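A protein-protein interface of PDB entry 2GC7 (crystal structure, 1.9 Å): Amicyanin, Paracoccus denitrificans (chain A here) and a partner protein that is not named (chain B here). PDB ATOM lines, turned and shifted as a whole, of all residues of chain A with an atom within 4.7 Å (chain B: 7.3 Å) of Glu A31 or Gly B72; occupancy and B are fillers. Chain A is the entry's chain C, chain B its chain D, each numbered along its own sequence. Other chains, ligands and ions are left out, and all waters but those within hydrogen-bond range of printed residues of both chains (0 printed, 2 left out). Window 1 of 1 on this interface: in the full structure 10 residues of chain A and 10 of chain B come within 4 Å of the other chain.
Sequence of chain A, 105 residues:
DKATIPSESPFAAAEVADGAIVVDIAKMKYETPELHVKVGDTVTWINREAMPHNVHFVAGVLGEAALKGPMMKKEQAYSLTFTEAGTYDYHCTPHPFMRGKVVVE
The side-chain carboxylate (OE1) of Glu A31 lies close to the side-chain carboxylate (OD1) of Asp B75. The side-chain hydroxyl (OG1) of Thr B79 is in hydrogen-bond range of the side-chain carboxylate (OD2) of Asp A24, 3.3 Å away. The backbone carbonyl oxygen (O) of Glu A31 sits at hydrogen-bond distance from the backbone NH (N) of Gly B72 (2.8 Å).
O of His B61 is in hydrogen-bond range of N of Glu B66 (3.5 Å). A ring nitrogen (ND1) of His B61 lies within hydrogen-bond range of the backbone carbonyl oxygen (O) of Pro B71, 2.5 Å away. O of His B61 is in hydrogen-bond range of N of Gly B67 (2.7 Å). The side-chain carboxylate of Glu B66 is in hydrogen-bond range of the backbone NH of Tyr B64, 2.8 Å away. O of Cys B60 lies within hydrogen-bond range of N of Ile B69 (3.3 Å). The backbone NH (N) of Tyr B77 lies within hydrogen-bond range of the side-chain carboxylate (OD2) of Asp B75, 2.9 Å away.
Asp A24 touches Tyr B77. Ala A26 touches Tyr B77. Lys A29 touches Glu B66 (NZ to O, 3.7 Å). Lys A29 touches Asp B75 (CD to OD1, 3.5 Å). Glu A31 touches Tyr B77. Lys B68 touches Thr A32. Thr A32 touches Ile B69. Pro B71 touches Thr A32. Pro A33 touches Gly B67. Pro A33 touches Lys B68 (CD to O, 3.7 Å).
Glu A31 touches just these residues of chain B: Pro B71, Gly B72, Asp B75 and Tyr B77. Printed residues of chain A within 4 Å of Asp B75: Lys A29 (3.5 Å) and Glu A31 (2.7 Å). Printed residues of chain A within 4 Å of Gly B67: Pro A33 (3.1 Å). Of the printed residues of chain B, Asp A24 touches Tyr B77 (3.5 Å) and Thr B79 (3.3 Å). Of the printed residues of chain B, Lys A29 touches Glu B66 and Asp B75. Printed residues of chain A within 4 Å of Lys B68: Thr A32 (3.6 Å) and Pro A33 (3.7 Å). Gly B62 touches none of the printed residues of chain A. Val A23 touches none of the printed residues of chain B. The nearest residue of chain B that does not touch Glu A31 is Gly B70 (4.2 Å). The nearest printed residue of chain A that does not touch Thr B79 is Glu A31 (6.6 Å).
Printed residues of chain B that touch a printed residue of chain A: Glu B66, Gly B67, Lys B68, Ile B69, Pro B71, Gly B72, Asp B75, Tyr B77 and Thr B79. Hydrophobic or aromatic side chains of chain B within 4 Å of the printed part of chain A: Pro B71 and Tyr B77. Among the printed residues, 14 pairs touch across the chains. Among the printed residues, no Asp or Glu carboxylate lies within 4 Å of a Lys or Arg side-chain nitrogen of the other chain.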
ATOM      1  N   VAL A  23      13.887  25.113 -17.130  1.00  0.00           N
ATOM      2  CA  VAL A  23      14.753  23.991 -16.773  1.00  0.00           C
ATOM      3  C   VAL A  23      14.828  23.127 -18.033  1.00  0.00           C
ATOM      4  O   VAL A  23      13.824  22.540 -18.443  1.00  0.00           O
ATOM      5  CB  VAL A  23      14.167  23.133 -15.623  1.00  0.00           C
ATOM      6  CG1 VAL A  23      15.037  21.893 -15.406  1.00  0.00           C
ATOM      7  CG2 VAL A  23      14.094  23.944 -14.339  1.00  0.00           C
ATOM      8  N   ASP A  24      15.996  23.064 -18.664  1.00  0.00           N
ATOM      9  CA  ASP A  24      16.141  22.264 -19.873  1.00  0.00           C
ATOM     10  C   ASP A  24      16.371  20.795 -19.540  1.00  0.00           C
ATOM     11  O   ASP A  24      17.063  20.465 -18.574  1.00  0.00           O
ATOM     12  CB  ASP A  24      17.319  22.754 -20.724  1.00  0.00           C
ATOM     13  CG  ASP A  24      17.103  24.149 -21.281  1.00  0.00           C
ATOM     14  OD1 ASP A  24      16.111  24.360 -22.007  1.00  0.00           O
ATOM     15  OD2 ASP A  24      17.941  25.029 -20.994  1.00  0.00           O
ATOM     16  N   ALA A  26      17.890  17.404 -21.145  1.00  0.00           N
ATOM     17  CA  ALA A  26      18.697  16.875 -22.236  1.00  0.00           C
ATOM     18  C   ALA A  26      19.720  15.888 -21.706  1.00  0.00           C
ATOM     19  O   ALA A  26      20.134  15.972 -20.551  1.00  0.00           O
ATOM     20  CB  ALA A  26      19.402  18.016 -22.966  1.00  0.00           C
ATOM     21  N   LYS A  29      18.929  14.112 -18.322  1.00  0.00           N
ATOM     22  CA  LYS A  29      19.061  14.878 -17.087  1.00  0.00           C
ATOM     23  C   LYS A  29      18.377  16.236 -17.126  1.00  0.00           C
ATOM     24  O   LYS A  29      18.158  16.808 -18.191  1.00  0.00           O
ATOM     25  CB  LYS A  29      20.545  15.087 -16.746  1.00  0.00           C
ATOM     26  CG  LYS A  29      21.323  15.872 -17.799  1.00  0.00           C
ATOM     27  CD  LYS A  29      22.833  15.877 -17.533  1.00  0.00           C
ATOM     28  CE  LYS A  29      23.271  17.062 -16.683  1.00  0.00           C
ATOM     29  NZ  LYS A  29      22.643  17.084 -15.333  1.00  0.00           N
ATOM     30  N   TYR A  30      18.017  16.728 -15.943  1.00  0.00           N
ATOM     31  CA  TYR A  30      17.421  18.049 -15.808  1.00  0.00           C
ATOM     32  C   TYR A  30      18.685  18.898 -15.667  1.00  0.00           C
ATOM     33  O   TYR A  30      19.411  18.762 -14.687  1.00  0.00           O
ATOM     34  CB  TYR A  30      16.562  18.112 -14.543  1.00  0.00           C
ATOM     35  CG  TYR A  30      15.372  17.169 -14.585  1.00  0.00           C
ATOM     36  CD1 TYR A  30      14.351  17.344 -15.525  1.00  0.00           C
ATOM     37  CD2 TYR A  30      15.279  16.087 -13.705  1.00  0.00           C
ATOM     38  CE1 TYR A  30      13.264  16.462 -15.592  1.00  0.00           C
ATOM     39  CE2 TYR A  30      14.193  15.198 -13.762  1.00  0.00           C
ATOM     40  CZ  TYR A  30      13.193  15.393 -14.706  1.00  0.00           C
ATOM     41  OH  TYR A  30      12.119  14.528 -14.761  1.00  0.00           O
ATOM     42  N   GLU A  31      18.960  19.741 -16.659  1.00  0.00           N
ATOM     43  CA  GLU A  31      20.182  20.550 -16.660  1.00  0.00           C
ATOM     44  C   GLU A  31      20.410  21.454 -15.446  1.00  0.00           C
ATOM     45  O   GLU A  31      21.553  21.780 -15.130  1.00  0.00           O
ATOM     46  CB  GLU A  31      20.271  21.349 -17.962  1.00  0.00           C
ATOM     47  CG  GLU A  31      20.450  20.470 -19.207  1.00  0.00           C
ATOM     48  CD  GLU A  31      21.774  19.704 -19.222  1.00  0.00           C
ATOM     49  OE1 GLU A  31      22.012  18.934 -20.174  1.00  0.00           O
ATOM     50  OE2 GLU A  31      22.586  19.875 -18.291  1.00  0.00           O
ATOM     51  N   THR A  32      19.338  21.864 -14.774  1.00  0.00           N
ATOM     52  CA  THR A  32      19.460  22.681 -13.565  1.00  0.00           C
ATOM     53  C   THR A  32      18.798  21.857 -12.455  1.00  0.00           C
ATOM     54  O   THR A  32      17.601  21.978 -12.204  1.00  0.00           O
ATOM     55  CB  THR A  32      18.737  24.043 -13.705  1.00  0.00           C
ATOM     56  OG1 THR A  32      19.279  24.767 -14.818  1.00  0.00           O
ATOM     57  CG2 THR A  32      18.939  24.873 -12.449  1.00  0.00           C
ATOM     58  N   PRO A  33      19.582  21.002 -11.782  1.00  0.00           N
ATOM     59  CA  PRO A  33      19.151  20.111 -10.698  1.00  0.00           C
ATOM     60  C   PRO A  33      18.567  20.724  -9.427  1.00  0.00           C
ATOM     61  O   PRO A  33      17.700  20.121  -8.796  1.00  0.00           O
ATOM     62  CB  PRO A  33      20.405  19.286 -10.418  1.00  0.00           C
ATOM     63  CG  PRO A  33      21.502  20.257 -10.698  1.00  0.00           C
ATOM     64  CD  PRO A  33      21.039  20.900 -11.986  1.00  0.00           C
ATOM     65  N   CYS B  60      27.611  28.250  -8.515  1.00  0.00           N
ATOM     66  CA  CYS B  60      26.378  28.200  -9.287  1.00  0.00           C
ATOM     67  C   CYS B  60      26.251  27.019 -10.235  1.00  0.00           C
ATOM     68  O   CYS B  60      25.159  26.480 -10.409  1.00  0.00           O
ATOM     69  CB  CYS B  60      26.203  29.480 -10.100  1.00  0.00           C
ATOM     70  SG  CYS B  60      25.936  30.993  -9.123  1.00  0.00           S
ATOM     71  N   HIS B  61      27.362  26.631 -10.854  1.00  0.00           N
ATOM     72  CA  HIS B  61      27.359  25.547 -11.827  1.00  0.00           C
ATOM     73  C   HIS B  61      27.765  24.173 -11.300  1.00  0.00           C
ATOM     74  O   HIS B  61      27.749  23.192 -12.043  1.00  0.00           O
ATOM     75  CB  HIS B  61      28.234  25.940 -13.022  1.00  0.00           C
ATOM     76  CG  HIS B  61      27.622  27.004 -13.882  1.00  0.00           C
ATOM     77  ND1 HIS B  61      26.504  26.750 -14.624  1.00  0.00           N
ATOM     78  CD2 HIS B  61      28.168  28.240 -13.889  1.00  0.00           C
ATOM     79  CE1 HIS B  61      26.285  27.991 -15.185  1.00  0.00           C
ATOM     80  NE2 HIS B  61      27.289  28.908 -14.748  1.00  0.00           N
ATOM     81  N   GLY B  62      28.125  24.099 -10.024  1.00  0.00           N
ATOM     82  CA  GLY B  62      28.503  22.821  -9.449  1.00  0.00           C
ATOM     83  C   GLY B  62      30.000  22.595  -9.407  1.00  0.00           C
ATOM     84  O   GLY B  62      30.749  23.131 -10.225  1.00  0.00           O
ATOM     85  N   TYR B  64      31.737  20.103 -10.295  1.00  0.00           N
ATOM     86  CA  TYR B  64      32.230  19.498 -11.529  1.00  0.00           C
ATOM     87  C   TYR B  64      31.437  19.941 -12.755  1.00  0.00           C
ATOM     88  O   TYR B  64      31.368  19.222 -13.753  1.00  0.00           O
ATOM     89  CB  TYR B  64      32.182  17.973 -11.412  1.00  0.00           C
ATOM     90  CG  TYR B  64      32.972  17.439 -10.238  1.00  0.00           C
ATOM     91  CD1 TYR B  64      34.346  17.647 -10.152  1.00  0.00           C
ATOM     92  CD2 TYR B  64      32.344  16.733  -9.213  1.00  0.00           C
ATOM     93  CE1 TYR B  64      35.079  17.164  -9.075  1.00  0.00           C
ATOM     94  CE2 TYR B  64      33.067  16.246  -8.129  1.00  0.00           C
ATOM     95  CZ  TYR B  64      34.434  16.465  -8.066  1.00  0.00           C
ATOM     96  OH  TYR B  64      35.160  15.998  -6.996  1.00  0.00           O
ATOM     97  N   ALA B  65      30.840  21.126 -12.673  1.00  0.00           N
ATOM     98  CA  ALA B  65      30.054  21.671 -13.772  1.00  0.00           C
ATOM     99  C   ALA B  65      28.872  20.774 -14.134  1.00  0.00           C
ATOM    100  O   ALA B  65      28.398  20.795 -15.270  1.00  0.00           O
ATOM    101  CB  ALA B  65      30.944  21.884 -14.992  1.00  0.00           C
ATOM    102  N   GLU B  66      28.400  19.992 -13.170  1.00  0.00           N
ATOM    103  CA  GLU B  66      27.260  19.111 -13.402  1.00  0.00           C
ATOM    104  C   GLU B  66      25.968  19.906 -13.221  1.00  0.00           C
ATOM    105  O   GLU B  66      24.879  19.405 -13.493  1.00  0.00           O
ATOM    106  CB  GLU B  66      27.270  17.936 -12.415  1.00  0.00           C
ATOM    107  CG  GLU B  66      27.002  18.335 -10.965  1.00  0.00           C
ATOM    108  CD  GLU B  66      28.249  18.787 -10.229  1.00  0.00           C
ATOM    109  OE1 GLU B  66      29.079  19.508 -10.827  1.00  0.00           O
ATOM    110  OE2 GLU B  66      28.392  18.430  -9.040  1.00  0.00           O
ATOM    111  N   GLY B  67      26.101  21.142 -12.744  1.00  0.00           N
ATOM    112  CA  GLY B  67      24.944  21.998 -12.532  1.00  0.00           C
ATOM    113  C   GLY B  67      24.424  21.978 -11.104  1.00  0.00           C
ATOM    114  O   GLY B  67      24.535  20.966 -10.415  1.00  0.00           O
ATOM    115  N   LYS B  68      23.876  23.103 -10.652  1.00  0.00           N
ATOM    116  CA  LYS B  68      23.307  23.206  -9.306  1.00  0.00           C
ATOM    117  C   LYS B  68      22.160  24.211  -9.357  1.00  0.00           C
ATOM    118  O   LYS B  68      21.049  23.847  -9.758  1.00  0.00           O
ATOM    119  CB  LYS B  68      24.350  23.652  -8.277  1.00  0.00           C
ATOM    120  CG  LYS B  68      23.841  23.516  -6.846  1.00  0.00           C
ATOM    121  CD  LYS B  68      24.748  24.157  -5.806  1.00  0.00           C
ATOM    122  CE  LYS B  68      26.122  23.516  -5.759  1.00  0.00           C
ATOM    123  NZ  LYS B  68      26.954  23.907  -6.928  1.00  0.00           N
ATOM    124  N   ILE B  69      22.399  25.459  -8.952  1.00  0.00           N
ATOM    125  CA  ILE B  69      21.327  26.450  -9.037  1.00  0.00           C
ATOM    126  C   ILE B  69      21.399  27.056 -10.426  1.00  0.00           C
ATOM    127  O   ILE B  69      20.489  27.753 -10.868  1.00  0.00           O
ATOM    128  CB  ILE B  69      21.430  27.581  -7.968  1.00  0.00           C
ATOM    129  CG1 ILE B  69      22.700  28.407  -8.165  1.00  0.00           C
ATOM    130  CG2 ILE B  69      21.389  26.976  -6.569  1.00  0.00           C
ATOM    131  CD1 ILE B  69      23.914  27.798  -7.531  1.00  0.00           C
ATOM    132  N   GLY B  70      22.501  26.765 -11.109  1.00  0.00           N
ATOM    133  CA  GLY B  70      22.712  27.229 -12.467  1.00  0.00           C
ATOM    134  C   GLY B  70      22.797  25.977 -13.325  1.00  0.00           C
ATOM    135  O   GLY B  70      22.979  24.891 -12.779  1.00  0.00           O
ATOM    136  N   PRO B  71      22.691  26.088 -14.659  1.00  0.00           N
ATOM    137  CA  PRO B  71      22.749  24.943 -15.576  1.00  0.00           C
ATOM    138  C   PRO B  71      24.089  24.218 -15.690  1.00  0.00           C
ATOM    139  O   PRO B  71      25.155  24.825 -15.557  1.00  0.00           O
ATOM    140  CB  PRO B  71      22.319  25.554 -16.906  1.00  0.00           C
ATOM    141  CG  PRO B  71      22.900  26.926 -16.820  1.00  0.00           C
ATOM    142  CD  PRO B  71      22.536  27.346 -15.411  1.00  0.00           C
ATOM    143  N   GLY B  72      24.021  22.913 -15.946  1.00  0.00           N
ATOM    144  CA  GLY B  72      25.226  22.119 -16.099  1.00  0.00           C
ATOM    145  C   GLY B  72      25.998  22.576 -17.324  1.00  0.00           C
ATOM    146  O   GLY B  72      25.418  23.147 -18.245  1.00  0.00           O
ATOM    147  N   LEU B  73      27.306  22.335 -17.339  1.00  0.00           N
ATOM    148  CA  LEU B  73      28.135  22.750 -18.468  1.00  0.00           C
ATOM    149  C   LEU B  73      29.028  21.605 -18.924  1.00  0.00           C
ATOM    150  O   LEU B  73      29.959  21.822 -19.698  1.00  0.00           O
ATOM    151  CB  LEU B  73      29.039  23.919 -18.056  1.00  0.00           C
ATOM    152  CG  LEU B  73      28.430  25.089 -17.272  1.00  0.00           C
ATOM    153  CD1 LEU B  73      29.546  25.984 -16.764  1.00  0.00           C
ATOM    154  CD2 LEU B  73      27.467  25.871 -18.147  1.00  0.00           C
ATOM    155  N   ASN B  74      28.744  20.390 -18.463  1.00  0.00           N
ATOM    156  CA  ASN B  74      29.598  19.256 -18.798  1.00  0.00           C
ATOM    157  C   ASN B  74      29.128  18.267 -19.864  1.00  0.00           C
ATOM    158  O   ASN B  74      29.692  17.178 -19.973  1.00  0.00           O
ATOM    159  CB  ASN B  74      29.932  18.484 -17.524  1.00  0.00           C
ATOM    160  CG  ASN B  74      28.728  17.774 -16.946  1.00  0.00           C
ATOM    161  OD1 ASN B  74      27.607  17.939 -17.429  1.00  0.00           O
ATOM    162  ND2 ASN B  74      28.953  16.977 -15.907  1.00  0.00           N
ATOM    163  N   ASP B  75      28.110  18.623 -20.642  1.00  0.00           N
ATOM    164  CA  ASP B  75      27.647  17.723 -21.689  1.00  0.00           C
ATOM    165  C   ASP B  75      27.453  18.445 -23.013  1.00  0.00           C
ATOM    166  O   ASP B  75      27.664  19.654 -23.106  1.00  0.00           O
ATOM    167  CB  ASP B  75      26.368  16.982 -21.257  1.00  0.00           C
ATOM    168  CG  ASP B  75      25.174  17.900 -21.062  1.00  0.00           C
ATOM    169  OD1 ASP B  75      24.285  17.523 -20.270  1.00  0.00           O
ATOM    170  OD2 ASP B  75      25.112  18.971 -21.702  1.00  0.00           O
ATOM    171  N   ALA B  76      27.057  17.690 -24.035  1.00  0.00           N
ATOM    172  CA  ALA B  76      26.872  18.219 -25.382  1.00  0.00           C
ATOM    173  C   ALA B  76      25.727  19.203 -25.582  1.00  0.00           C
ATOM    174  O   ALA B  76      25.595  19.785 -26.658  1.00  0.00           O
ATOM    175  CB  ALA B  76      26.733  17.059 -26.371  1.00  0.00           C
ATOM    176  N   TYR B  77      24.891  19.396 -24.568  1.00  0.00           N
ATOM    177  CA  TYR B  77      23.790  20.334 -24.722  1.00  0.00           C
ATOM    178  C   TYR B  77      24.164  21.733 -24.254  1.00  0.00           C
ATOM    179  O   TYR B  77      24.757  21.899 -23.185  1.00  0.00           O
ATOM    180  CB  TYR B  77      22.548  19.883 -23.943  1.00  0.00           C
ATOM    181  CG  TYR B  77      21.443  20.911 -24.026  1.00  0.00           C
ATOM    182  CD1 TYR B  77      20.695  21.061 -25.194  1.00  0.00           C
ATOM    183  CD2 TYR B  77      21.216  21.806 -22.982  1.00  0.00           C
ATOM    184  CE1 TYR B  77      19.754  22.079 -25.329  1.00  0.00           C
ATOM    185  CE2 TYR B  77      20.275  22.833 -23.105  1.00  0.00           C
ATOM    186  CZ  TYR B  77      19.550  22.962 -24.283  1.00  0.00           C
ATOM    187  OH  TYR B  77      18.629  23.974 -24.421  1.00  0.00           O
ATOM    188  N   TRP B  78      23.807  22.735 -25.056  1.00  0.00           N
ATOM    189  CA  TRP B  78      24.075  24.130 -24.714  1.00  0.00           C
ATOM    190  C   TRP B  78      22.849  24.989 -25.002  1.00  0.00           C
ATOM    191  O   TRP B  78      22.275  24.919 -26.088  1.00  0.00           O
ATOM    192  CB  TRP B  78      25.261  24.680 -25.515  1.00  0.00           C
ATOM    193  CG  TRP B  78      26.562  23.968 -25.289  1.00  0.00           C
ATOM    194  CD1 TRP B  78      27.107  22.993 -26.072  1.00  0.00           C
ATOM    195  CD2 TRP B  78      27.483  24.181 -24.213  1.00  0.00           C
ATOM    196  NE1 TRP B  78      28.312  22.586 -25.554  1.00  0.00           N
ATOM    197  CE2 TRP B  78      28.568  23.298 -24.411  1.00  0.00           C
ATOM    198  CE3 TRP B  78      27.497  25.030 -23.098  1.00  0.00           C
ATOM    199  CZ2 TRP B  78      29.660  23.239 -23.536  1.00  0.00           C
ATOM    200  CZ3 TRP B  78      28.583  24.973 -22.227  1.00  0.00           C
ATOM    201  CH2 TRP B  78      29.649  24.081 -22.454  1.00  0.00           C
ATOM    202  N   THR B  79      22.448  25.794 -24.025  1.00  0.00           N
ATOM    203  CA  THR B  79      21.305  26.680 -24.191  1.00  0.00           C
ATOM    204  C   THR B  79      21.617  27.610 -25.351  1.00  0.00           C
ATOM    205  O   THR B  79      20.755  27.929 -26.170  1.00  0.00           O
ATOM    206  CB  THR B  79      21.070  27.507 -22.920  1.00  0.00           C
ATOM    207  OG1 THR B  79      20.691  26.627 -21.854  1.00  0.00           O
ATOM    208  CG2 THR B  79      19.977  28.545 -23.142  1.00  0.00           C
